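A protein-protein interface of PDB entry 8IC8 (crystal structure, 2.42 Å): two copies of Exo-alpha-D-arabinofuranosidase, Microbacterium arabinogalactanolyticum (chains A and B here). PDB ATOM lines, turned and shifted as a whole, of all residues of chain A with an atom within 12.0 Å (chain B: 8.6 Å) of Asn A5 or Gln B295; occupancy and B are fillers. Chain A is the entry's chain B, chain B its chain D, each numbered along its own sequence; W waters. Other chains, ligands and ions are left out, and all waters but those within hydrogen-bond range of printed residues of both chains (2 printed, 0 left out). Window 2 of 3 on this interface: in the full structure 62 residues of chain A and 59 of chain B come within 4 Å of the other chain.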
ATOM      1  N   PRO A   2     -20.347   2.174 -11.351  1.00  0.00           N
ATOM      2  CA  PRO A   2     -20.222   3.148 -10.258  1.00  0.00           C
ATOM      3  C   PRO A   2     -19.347   4.359 -10.612  1.00  0.00           C
ATOM      4  O   PRO A   2     -18.945   4.505 -11.759  1.00  0.00           O
ATOM      5  CB  PRO A   2     -19.580   2.327  -9.135  1.00  0.00           C
ATOM      6  CG  PRO A   2     -18.848   1.220  -9.835  1.00  0.00           C
ATOM      7  CD  PRO A   2     -19.390   1.058 -11.222  1.00  0.00           C
ATOM      8  N   ASP A   3     -19.078   5.217  -9.630  1.00  0.00           N
ATOM      9  CA  ASP A   3     -18.188   6.361  -9.787  1.00  0.00           C
ATOM     10  C   ASP A   3     -17.391   6.474  -8.486  1.00  0.00           C
ATOM     11  O   ASP A   3     -17.494   5.617  -7.610  1.00  0.00           O
ATOM     12  CB  ASP A   3     -18.976   7.642 -10.156  1.00  0.00           C
ATOM     13  CG  ASP A   3     -20.167   7.914  -9.217  1.00  0.00           C
ATOM     14  OD1 ASP A   3     -20.202   7.278  -8.149  1.00  0.00           O
ATOM     15  OD2 ASP A   3     -21.062   8.761  -9.509  1.00  0.00           O
ATOM     16  N   LEU A   4     -16.596   7.532  -8.351  1.00  0.00           N
ATOM     17  CA  LEU A   4     -15.731   7.665  -7.183  1.00  0.00           C
ATOM     18  C   LEU A   4     -16.539   7.685  -5.889  1.00  0.00           C
ATOM     19  O   LEU A   4     -16.141   7.069  -4.893  1.00  0.00           O
ATOM     20  CB  LEU A   4     -14.875   8.931  -7.313  1.00  0.00           C
ATOM     21  CG  LEU A   4     -13.896   9.193  -6.166  1.00  0.00           C
ATOM     22  CD1 LEU A   4     -12.740   8.214  -6.237  1.00  0.00           C
ATOM     23  CD2 LEU A   4     -13.379  10.623  -6.197  1.00  0.00           C
ATOM     24  N   ASN A   5     -17.688   8.365  -5.889  1.00  0.00           N
ATOM     25  CA  ASN A   5     -18.563   8.390  -4.712  1.00  0.00           C
ATOM     26  C   ASN A   5     -19.136   7.011  -4.371  1.00  0.00           C
ATOM     27  O   ASN A   5     -19.359   6.712  -3.198  1.00  0.00           O
ATOM     28  CB  ASN A   5     -19.710   9.382  -4.930  1.00  0.00           C
ATOM     29  CG  ASN A   5     -20.745   9.342  -3.812  1.00  0.00           C
ATOM     30  OD1 ASN A   5     -20.399   9.434  -2.649  1.00  0.00           O
ATOM     31  ND2 ASN A   5     -22.020   9.221  -4.168  1.00  0.00           N
ATOM     32  N   SER A   6     -19.402   6.155  -5.357  1.00  0.00           N
ATOM     33  CA  SER A   6     -20.040   4.879  -5.060  1.00  0.00           C
ATOM     34  C   SER A   6     -19.111   3.679  -5.227  1.00  0.00           C
ATOM     35  O   SER A   6     -19.581   2.542  -5.168  1.00  0.00           O
ATOM     36  CB  SER A   6     -21.287   4.702  -5.926  1.00  0.00           C
ATOM     37  OG  SER A   6     -20.919   4.554  -7.280  1.00  0.00           O
ATOM     38  N   ILE A   7     -17.800   3.893  -5.389  1.00  0.00           N
ATOM     39  CA  ILE A   7     -16.941   2.801  -5.846  1.00  0.00           C
ATOM     40  C   ILE A   7     -16.734   1.732  -4.774  1.00  0.00           C
ATOM     41  O   ILE A   7     -16.449   0.578  -5.110  1.00  0.00           O
ATOM     42  CB  ILE A   7     -15.589   3.344  -6.363  1.00  0.00           C
ATOM     43  CG1 ILE A   7     -14.766   2.241  -7.062  1.00  0.00           C
ATOM     44  CG2 ILE A   7     -14.776   3.924  -5.236  1.00  0.00           C
ATOM     45  CD1 ILE A   7     -15.470   1.540  -8.208  1.00  0.00           C
ATOM     46  N   ALA A   8     -16.896   2.055  -3.491  1.00  0.00           N
ATOM     47  CA  ALA A   8     -16.549   1.083  -2.454  1.00  0.00           C
ATOM     48  C   ALA A   8     -17.602   0.003  -2.277  1.00  0.00           C
ATOM     49  O   ALA A   8     -17.312  -1.029  -1.666  1.00  0.00           O
ATOM     50  CB  ALA A   8     -16.336   1.768  -1.104  1.00  0.00           C
ATOM     51  N   ALA A   9     -18.812   0.224  -2.773  1.00  0.00           N
ATOM     52  CA  ALA A   9     -19.892  -0.723  -2.543  1.00  0.00           C
ATOM     53  C   ALA A   9     -19.582  -2.068  -3.188  1.00  0.00           C
ATOM     54  O   ALA A   9     -19.150  -2.138  -4.339  1.00  0.00           O
ATOM     55  CB  ALA A   9     -21.198  -0.156  -3.093  1.00  0.00           C
ATOM     56  N   LEU A  10     -19.811  -3.142  -2.443  1.00  0.00           N
ATOM     57  CA  LEU A  10     -19.750  -4.480  -3.019  1.00  0.00           C
ATOM     58  C   LEU A  10     -20.972  -4.734  -3.901  1.00  0.00           C
ATOM     59  O   LEU A  10     -22.110  -4.520  -3.474  1.00  0.00           O
ATOM     60  CB  LEU A  10     -19.687  -5.511  -1.899  1.00  0.00           C
ATOM     61  CG  LEU A  10     -18.406  -5.450  -1.069  1.00  0.00           C
ATOM     62  CD1 LEU A  10     -18.637  -6.070   0.314  1.00  0.00           C
ATOM     63  CD2 LEU A  10     -17.283  -6.156  -1.842  1.00  0.00           C
ATOM     64  N   ARG A  11     -20.741  -5.186  -5.131  1.00  0.00           N
ATOM     65  CA  ARG A  11     -21.813  -5.488  -6.075  1.00  0.00           C
ATOM     66  C   ARG A  11     -21.595  -6.858  -6.712  1.00  0.00           C
ATOM     67  O   ARG A  11     -20.453  -7.252  -6.965  1.00  0.00           O
ATOM     68  CB  ARG A  11     -21.880  -4.419  -7.176  1.00  0.00           C
ATOM     69  CG  ARG A  11     -21.652  -3.006  -6.674  1.00  0.00           C
ATOM     70  CD  ARG A  11     -21.382  -2.044  -7.807  1.00  0.00           C
ATOM     71  NE  ARG A  11     -22.447  -1.048  -7.819  1.00  0.00           N
ATOM     72  CZ  ARG A  11     -22.454   0.085  -7.128  1.00  0.00           C
ATOM     73  NH1 ARG A  11     -23.517   0.866  -7.205  1.00  0.00           N
ATOM     74  NH2 ARG A  11     -21.421   0.445  -6.377  1.00  0.00           N
ATOM     75  N   GLN A 124     -15.038  14.092 -19.154  1.00  0.00           N
ATOM     76  CA  GLN A 124     -15.469  12.965 -18.336  1.00  0.00           C
ATOM     77  C   GLN A 124     -15.903  11.784 -19.195  1.00  0.00           C
ATOM     78  O   GLN A 124     -15.587  10.628 -18.887  1.00  0.00           O
ATOM     79  CB  GLN A 124     -16.631  13.406 -17.439  1.00  0.00           C
ATOM     80  CG  GLN A 124     -16.758  12.586 -16.150  1.00  0.00           C
ATOM     81  CD  GLN A 124     -15.883  13.131 -15.046  1.00  0.00           C
ATOM     82  OE1 GLN A 124     -15.804  14.350 -14.851  1.00  0.00           O
ATOM     83  NE2 GLN A 124     -15.220  12.246 -14.317  1.00  0.00           N
ATOM     84  N   PRO A 267     -14.545  19.081 -17.803  1.00  0.00           N
ATOM     85  CA  PRO A 267     -15.378  17.868 -17.738  1.00  0.00           C
ATOM     86  C   PRO A 267     -16.551  17.838 -18.707  1.00  0.00           C
ATOM     87  O   PRO A 267     -16.808  16.780 -19.300  1.00  0.00           O
ATOM     88  CB  PRO A 267     -15.842  17.866 -16.279  1.00  0.00           C
ATOM     89  CG  PRO A 267     -14.749  18.490 -15.577  1.00  0.00           C
ATOM     90  CD  PRO A 267     -14.287  19.599 -16.445  1.00  0.00           C
ATOM     91  N   TYR A 268     -17.279  18.946 -18.891  1.00  0.00           N
ATOM     92  CA  TYR A 268     -18.461  18.925 -19.755  1.00  0.00           C
ATOM     93  C   TYR A 268     -18.374  19.857 -20.956  1.00  0.00           C
ATOM     94  O   TYR A 268     -19.305  19.879 -21.773  1.00  0.00           O
ATOM     95  CB  TYR A 268     -19.716  19.277 -18.944  1.00  0.00           C
ATOM     96  CG  TYR A 268     -19.750  18.560 -17.621  1.00  0.00           C
ATOM     97  CD1 TYR A 268     -19.774  17.165 -17.573  1.00  0.00           C
ATOM     98  CD2 TYR A 268     -19.728  19.262 -16.414  1.00  0.00           C
ATOM     99  CE1 TYR A 268     -19.797  16.495 -16.393  1.00  0.00           C
ATOM    100  CE2 TYR A 268     -19.745  18.582 -15.207  1.00  0.00           C
ATOM    101  CZ  TYR A 268     -19.783  17.195 -15.211  1.00  0.00           C
ATOM    102  OH  TYR A 268     -19.794  16.493 -14.031  1.00  0.00           O
ATOM    103  N   GLN A 295     -24.687  16.429 -15.963  1.00  0.00           N
ATOM    104  CA  GLN A 295     -25.424  17.003 -14.838  1.00  0.00           C
ATOM    105  C   GLN A 295     -26.680  17.731 -15.284  1.00  0.00           C
ATOM    106  O   GLN A 295     -27.610  17.882 -14.489  1.00  0.00           O
ATOM    107  CB  GLN A 295     -24.557  17.990 -14.054  1.00  0.00           C
ATOM    108  CG  GLN A 295     -23.217  17.434 -13.585  1.00  0.00           C
ATOM    109  CD  GLN A 295     -23.334  16.609 -12.307  1.00  0.00           C
ATOM    110  OE1 GLN A 295     -24.232  16.838 -11.475  1.00  0.00           O
ATOM    111  NE2 GLN A 295     -22.427  15.643 -12.143  1.00  0.00           N
ATOM    112  N   ASP B   3     -25.172  11.932 -13.211  1.00  0.00           N
ATOM    113  CA  ASP B   3     -23.759  12.068 -13.565  1.00  0.00           C
ATOM    114  C   ASP B   3     -23.451  10.981 -14.598  1.00  0.00           C
ATOM    115  O   ASP B   3     -24.349  10.281 -15.079  1.00  0.00           O
ATOM    116  CB  ASP B   3     -22.854  12.033 -12.310  1.00  0.00           C
ATOM    117  CG  ASP B   3     -23.126  10.831 -11.384  1.00  0.00           C
ATOM    118  OD1 ASP B   3     -23.840   9.919 -11.846  1.00  0.00           O
ATOM    119  OD2 ASP B   3     -22.613  10.777 -10.205  1.00  0.00           O
ATOM    120  N   ASN B   5     -22.053   8.110 -14.256  1.00  0.00           N
ATOM    121  CA  ASN B   5     -22.421   6.789 -13.761  1.00  0.00           C
ATOM    122  C   ASN B   5     -23.928   6.539 -13.831  1.00  0.00           C
ATOM    123  O   ASN B   5     -24.353   5.406 -14.066  1.00  0.00           O
ATOM    124  CB  ASN B   5     -21.923   6.618 -12.324  1.00  0.00           C
ATOM    125  CG  ASN B   5     -22.398   5.327 -11.698  1.00  0.00           C
ATOM    126  OD1 ASN B   5     -22.235   4.243 -12.277  1.00  0.00           O
ATOM    127  ND2 ASN B   5     -22.996   5.424 -10.521  1.00  0.00           N
ATOM    128  N   GLN B 124     -15.039  20.660 -11.350  1.00  0.00           N
ATOM    129  CA  GLN B 124     -16.284  19.929 -11.555  1.00  0.00           C
ATOM    130  C   GLN B 124     -17.481  20.869 -11.480  1.00  0.00           C
ATOM    131  O   GLN B 124     -18.388  20.800 -12.323  1.00  0.00           O
ATOM    132  CB  GLN B 124     -16.415  18.804 -10.509  1.00  0.00           C
ATOM    133  CG  GLN B 124     -17.220  17.578 -11.013  1.00  0.00           C
ATOM    134  CD  GLN B 124     -16.402  16.715 -11.971  1.00  0.00           C
ATOM    135  OE1 GLN B 124     -15.201  16.532 -11.776  1.00  0.00           O
ATOM    136  NE2 GLN B 124     -17.043  16.202 -13.010  1.00  0.00           N
ATOM    137  N   TYR B 206     -20.898  22.398   4.349  1.00  0.00           N
ATOM    138  CA  TYR B 206     -20.021  23.341   3.668  1.00  0.00           C
ATOM    139  C   TYR B 206     -19.361  22.641   2.487  1.00  0.00           C
ATOM    140  O   TYR B 206     -18.824  21.541   2.647  1.00  0.00           O
ATOM    141  CB  TYR B 206     -18.974  23.844   4.661  1.00  0.00           C
ATOM    142  CG  TYR B 206     -18.142  25.019   4.199  1.00  0.00           C
ATOM    143  CD1 TYR B 206     -17.124  24.858   3.247  1.00  0.00           C
ATOM    144  CD2 TYR B 206     -18.342  26.291   4.744  1.00  0.00           C
ATOM    145  CE1 TYR B 206     -16.344  25.948   2.827  1.00  0.00           C
ATOM    146  CE2 TYR B 206     -17.573  27.382   4.337  1.00  0.00           C
ATOM    147  CZ  TYR B 206     -16.575  27.207   3.381  1.00  0.00           C
ATOM    148  OH  TYR B 206     -15.814  28.291   2.994  1.00  0.00           O
ATOM    149  N   VAL B 207     -19.389  23.261   1.302  1.00  0.00           N
ATOM    150  CA  VAL B 207     -18.963  22.580   0.083  1.00  0.00           C
ATOM    151  C   VAL B 207     -18.002  23.391  -0.768  1.00  0.00           C
ATOM    152  O   VAL B 207     -17.579  22.910  -1.825  1.00  0.00           O
ATOM    153  CB  VAL B 207     -20.168  22.148  -0.778  1.00  0.00           C
ATOM    154  CG1 VAL B 207     -20.981  21.085  -0.056  1.00  0.00           C
ATOM    155  CG2 VAL B 207     -21.017  23.345  -1.154  1.00  0.00           C
ATOM    156  N   PRO B 267     -10.353  18.794 -10.438  1.00  0.00           N
ATOM    157  CA  PRO B 267     -11.811  18.761 -10.184  1.00  0.00           C
ATOM    158  C   PRO B 267     -12.253  19.461  -8.906  1.00  0.00           C
ATOM    159  O   PRO B 267     -13.281  20.155  -8.923  1.00  0.00           O
ATOM    160  CB  PRO B 267     -12.117  17.257 -10.135  1.00  0.00           C
ATOM    161  CG  PRO B 267     -11.108  16.657 -11.059  1.00  0.00           C
ATOM    162  CD  PRO B 267      -9.853  17.473 -10.883  1.00  0.00           C
ATOM    163  N   TYR B 268     -11.521  19.303  -7.802  1.00  0.00           N
ATOM    164  CA  TYR B 268     -11.928  19.861  -6.518  1.00  0.00           C
ATOM    165  C   TYR B 268     -10.974  20.910  -5.963  1.00  0.00           C
ATOM    166  O   TYR B 268     -11.335  21.593  -5.004  1.00  0.00           O
ATOM    167  CB  TYR B 268     -12.082  18.742  -5.474  1.00  0.00           C
ATOM    168  CG  TYR B 268     -12.846  17.560  -6.012  1.00  0.00           C
ATOM    169  CD1 TYR B 268     -14.126  17.731  -6.513  1.00  0.00           C
ATOM    170  CD2 TYR B 268     -12.285  16.279  -6.047  1.00  0.00           C
ATOM    171  CE1 TYR B 268     -14.847  16.681  -7.015  1.00  0.00           C
ATOM    172  CE2 TYR B 268     -13.010  15.207  -6.553  1.00  0.00           C
ATOM    173  CZ  TYR B 268     -14.302  15.426  -7.030  1.00  0.00           C
ATOM    174  OH  TYR B 268     -15.067  14.423  -7.552  1.00  0.00           O
ATOM    175  N   ARG B 291     -11.519  25.581  -3.598  1.00  0.00           N
ATOM    176  CA  ARG B 291     -11.611  24.198  -3.147  1.00  0.00           C
ATOM    177  C   ARG B 291     -13.082  23.834  -3.003  1.00  0.00           C
ATOM    178  O   ARG B 291     -13.817  24.504  -2.260  1.00  0.00           O
ATOM    179  CB  ARG B 291     -10.894  23.975  -1.813  1.00  0.00           C
ATOM    180  CG  ARG B 291     -11.273  22.614  -1.194  1.00  0.00           C
ATOM    181  CD  ARG B 291     -10.298  22.152  -0.131  1.00  0.00           C
ATOM    182  NE  ARG B 291     -10.623  20.817   0.348  1.00  0.00           N
ATOM    183  CZ  ARG B 291     -10.032  20.241   1.386  1.00  0.00           C
ATOM    184  NH1 ARG B 291      -9.078  20.897   2.044  1.00  0.00           N
ATOM    185  NH2 ARG B 291     -10.383  19.014   1.765  1.00  0.00           N
ATOM    186  N   TRP B 292     -13.504  22.779  -3.707  1.00  0.00           N
ATOM    187  CA  TRP B 292     -14.842  22.231  -3.559  1.00  0.00           C
ATOM    188  C   TRP B 292     -14.780  20.993  -2.664  1.00  0.00           C
ATOM    189  O   TRP B 292     -13.913  20.129  -2.839  1.00  0.00           O
ATOM    190  CB  TRP B 292     -15.459  21.893  -4.918  1.00  0.00           C
ATOM    191  CG  TRP B 292     -15.327  22.967  -5.989  1.00  0.00           C
ATOM    192  CD1 TRP B 292     -15.066  22.752  -7.311  1.00  0.00           C
ATOM    193  CD2 TRP B 292     -15.458  24.400  -5.838  1.00  0.00           C
ATOM    194  NE1 TRP B 292     -15.023  23.947  -7.990  1.00  0.00           N
ATOM    195  CE2 TRP B 292     -15.255  24.974  -7.113  1.00  0.00           C
ATOM    196  CE3 TRP B 292     -15.718  25.249  -4.754  1.00  0.00           C
ATOM    197  CZ2 TRP B 292     -15.311  26.367  -7.338  1.00  0.00           C
ATOM    198  CZ3 TRP B 292     -15.772  26.636  -4.978  1.00  0.00           C
ATOM    199  CH2 TRP B 292     -15.570  27.177  -6.259  1.00  0.00           C
ATOM    200  N   HIS B 293     -15.672  20.936  -1.675  1.00  0.00           N
ATOM    201  CA  HIS B 293     -15.764  19.787  -0.778  1.00  0.00           C
ATOM    202  C   HIS B 293     -16.966  18.991  -1.272  1.00  0.00           C
ATOM    203  O   HIS B 293     -18.072  19.081  -0.743  1.00  0.00           O
ATOM    204  CB  HIS B 293     -15.915  20.215   0.687  1.00  0.00           C
ATOM    205  CG  HIS B 293     -14.814  21.097   1.201  1.00  0.00           C
ATOM    206  ND1 HIS B 293     -13.925  20.687   2.173  1.00  0.00           N
ATOM    207  CD2 HIS B 293     -14.482  22.379   0.911  1.00  0.00           C
ATOM    208  CE1 HIS B 293     -13.088  21.670   2.452  1.00  0.00           C
ATOM    209  NE2 HIS B 293     -13.406  22.711   1.706  1.00  0.00           N
ATOM    210  N   LEU B 294     -16.748  18.226  -2.337  1.00  0.00           N
ATOM    211  CA  LEU B 294     -17.830  17.505  -2.988  1.00  0.00           C
ATOM    212  C   LEU B 294     -17.869  16.047  -2.556  1.00  0.00           C
ATOM    213  O   LEU B 294     -18.919  15.558  -2.125  1.00  0.00           O
ATOM    214  CB  LEU B 294     -17.680  17.621  -4.511  1.00  0.00           C
ATOM    215  CG  LEU B 294     -18.085  18.954  -5.142  1.00  0.00           C
ATOM    216  CD1 LEU B 294     -17.949  18.886  -6.661  1.00  0.00           C
ATOM    217  CD2 LEU B 294     -19.509  19.355  -4.742  1.00  0.00           C
ATOM    218  N   GLN B 295     -16.736  15.341  -2.655  1.00  0.00           N
ATOM    219  CA  GLN B 295     -16.632  14.008  -2.081  1.00  0.00           C
ATOM    220  C   GLN B 295     -16.426  14.058  -0.569  1.00  0.00           C
ATOM    221  O   GLN B 295     -16.661  13.050   0.112  1.00  0.00           O
ATOM    222  CB  GLN B 295     -15.490  13.239  -2.749  1.00  0.00           C
ATOM    223  CG  GLN B 295     -15.558  13.243  -4.277  1.00  0.00           C
ATOM    224  CD  GLN B 295     -16.351  12.065  -4.837  1.00  0.00           C
ATOM    225  OE1 GLN B 295     -16.477  11.022  -4.195  1.00  0.00           O
ATOM    226  NE2 GLN B 295     -16.897  12.234  -6.030  1.00  0.00           N
ATOM    227  N   ASP B 296     -16.018  15.212  -0.036  1.00  0.00           N
ATOM    228  CA  ASP B 296     -15.713  15.377   1.387  1.00  0.00           C
ATOM    229  C   ASP B 296     -16.373  16.634   1.944  1.00  0.00           C
ATOM    230  O   ASP B 296     -15.695  17.535   2.454  1.00  0.00           O
ATOM    231  CB  ASP B 296     -14.201  15.432   1.596  1.00  0.00           C
ATOM    232  CG  ASP B 296     -13.536  16.537   0.765  1.00  0.00           C
ATOM    233  OD1 ASP B 296     -13.945  16.741  -0.392  1.00  0.00           O
ATOM    234  OD2 ASP B 296     -12.611  17.200   1.274  1.00  0.00           O
ATOM    235  N   PRO B 297     -17.700  16.730   1.870  1.00  0.00           N
ATOM    236  CA  PRO B 297     -18.376  17.906   2.443  1.00  0.00           C
ATOM    237  C   PRO B 297     -18.098  18.005   3.936  1.00  0.00           C
ATOM    238  O   PRO B 297     -17.717  17.033   4.590  1.00  0.00           O
ATOM    239  CB  PRO B 297     -19.864  17.641   2.174  1.00  0.00           C
ATOM    240  CG  PRO B 297     -19.966  16.120   2.036  1.00  0.00           C
ATOM    241  CD  PRO B 297     -18.651  15.679   1.446  1.00  0.00           C
ATOM    242  N   ILE B 298     -18.277  19.198   4.487  1.00  0.00           N
ATOM    243  CA  ILE B 298     -18.084  19.388   5.919  1.00  0.00           C
ATOM    244  C   ILE B 298     -19.469  19.545   6.531  1.00  0.00           C
ATOM    245  O   ILE B 298     -20.087  20.610   6.446  1.00  0.00           O
ATOM    246  CB  ILE B 298     -17.161  20.567   6.234  1.00  0.00           C
ATOM    247  CG1 ILE B 298     -15.722  20.184   5.869  1.00  0.00           C
ATOM    248  CG2 ILE B 298     -17.252  20.933   7.713  1.00  0.00           C
ATOM    249  CD1 ILE B 298     -14.757  21.375   5.828  1.00  0.00           C
ATOM    250  N   HIS B 299     -19.957  18.464   7.137  1.00  0.00           N
ATOM    251  CA  HIS B 299     -21.326  18.398   7.640  1.00  0.00           C
ATOM    252  C   HIS B 299     -21.457  19.130   8.969  1.00  0.00           C
ATOM    253  O   HIS B 299     -20.506  19.218   9.757  1.00  0.00           O
ATOM    254  CB  HIS B 299     -21.754  16.941   7.823  1.00  0.00           C
ATOM    255  CG  HIS B 299     -22.215  16.279   6.560  1.00  0.00           C
ATOM    256  ND1 HIS B 299     -23.498  16.415   6.069  1.00  0.00           N
ATOM    257  CD2 HIS B 299     -21.564  15.477   5.686  1.00  0.00           C
ATOM    258  CE1 HIS B 299     -23.615  15.726   4.949  1.00  0.00           C
ATOM    259  NE2 HIS B 299     -22.456  15.146   4.694  1.00  0.00           N
HETATM  260  O   HOH W   1     -21.655  13.702  -9.827  1.00  0.00           O
HETATM  261  O   HOH W   2     -13.449  15.370 -13.774  1.00  0.00           O
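The backbone carbonyl oxygen (O) of Pro A2 sits close to the side-chain amide oxygen (OD1) of Asn B5.
The side-chain carboxylate of Asp A3 sits close to the side-chain carboxylate of Asp B3 (2.6 Å).
The backbone NH of Asn A5 sits at hydrogen-bond distance from the side-chain amide oxygen of Gln B295 (3.4 Å).
OE1 of Gln A124 sits at hydrogen-bond distance from NE2 of Gln B124, at 2.9 Å.
NE2 of Gln B124 is in hydrogen-bond range of OH of Tyr A268 (2.9 Å).
OD1 of Asp A3 sits at hydrogen-bond distance from OG of Ser A6, 2.9 Å away.
The guanidinium group of Arg A11 is in hydrogen-bond range of the backbone carbonyl oxygen of Ser A6 (3.0 Å).
O of Pro A267 is in hydrogen-bond range of N of Gln A124 (3.2 Å).
The side-chain hydroxyl (OH) of Tyr A268 is in hydrogen-bond range of the side-chain amide nitrogen (NE2) of Gln A295.
The backbone NH (N) of Gln B124 lies within hydrogen-bond range of the backbone carbonyl oxygen (O) of Pro B267.
OH of Tyr B268 is in hydrogen-bond range of NE2 of Gln B295 (3.2 Å).
Asn B5 touches Asp A3 (CB to OD2, 3.6 Å).
CD of Gln B295 touches CD2 of Leu A4, 3.6 Å away.
Asn B5 touches Ser A6 (ND2 to OG, 3.9 Å).
Pro A267 touches Gln B124.
Asp B3 touches Gln A295 (CB to NE2, 3.6 Å).
Of chain A, only Leu A4 (3.6 Å) and Asn A5 (3.4 Å) come within 4 Å of Gln B295.
No residue of chain A comes within 4 Å of Leu B294.
Pro B297 touches none of the printed residues of chain A.
Of the printed residues of chain A, Asp B3 touches Asp A3 and Gln A295.
Of the printed residues of chain B, Gln A295 touches Asp B3.
His B299 touches none of the printed residues of chain A.
The nearest residue of chain B that does not touch Asn A5 is Asp B3 (6.2 Å).
The nearest residue of chain A that does not touch Gln B295 is Ser A6 (5.8 Å).
Along chain B the printed residues that touch a printed residue of chain A span positions 3 to 295.
Hydrophobic or aromatic side chains of chain A that line the printed part of chain B: Leu A4, Pro A267 and Tyr A268.
Among the printed residues, 10 pairs touch across the chains.
Asp B3 touches its own counterpart, Asp A3.
Asn A5 touches Gln B295, but with the chains exchanged Gln A295 does not touch Asn B5 (7.8 Å).
Gln A124 touches its own counterpart, Gln B124.
Gln A295 touches Asp B3, but with the chains exchanged Asp A3 does not touch Gln B295 (6.3 Å).
Positions printed for both chains: 3, 5, 124, 267, 268 and 295.
Water W2 bridges OE1 of Gln A124 (2.8 Å) and OE1 of Gln B124 (2.9 Å).
Water W1 lies within hydrogen-bond range of the side-chain carboxylate (OD2) of Asp B3 (3.1 Å) and the side-chain amide nitrogen (NE2) of Gln A295 (3.1 Å).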
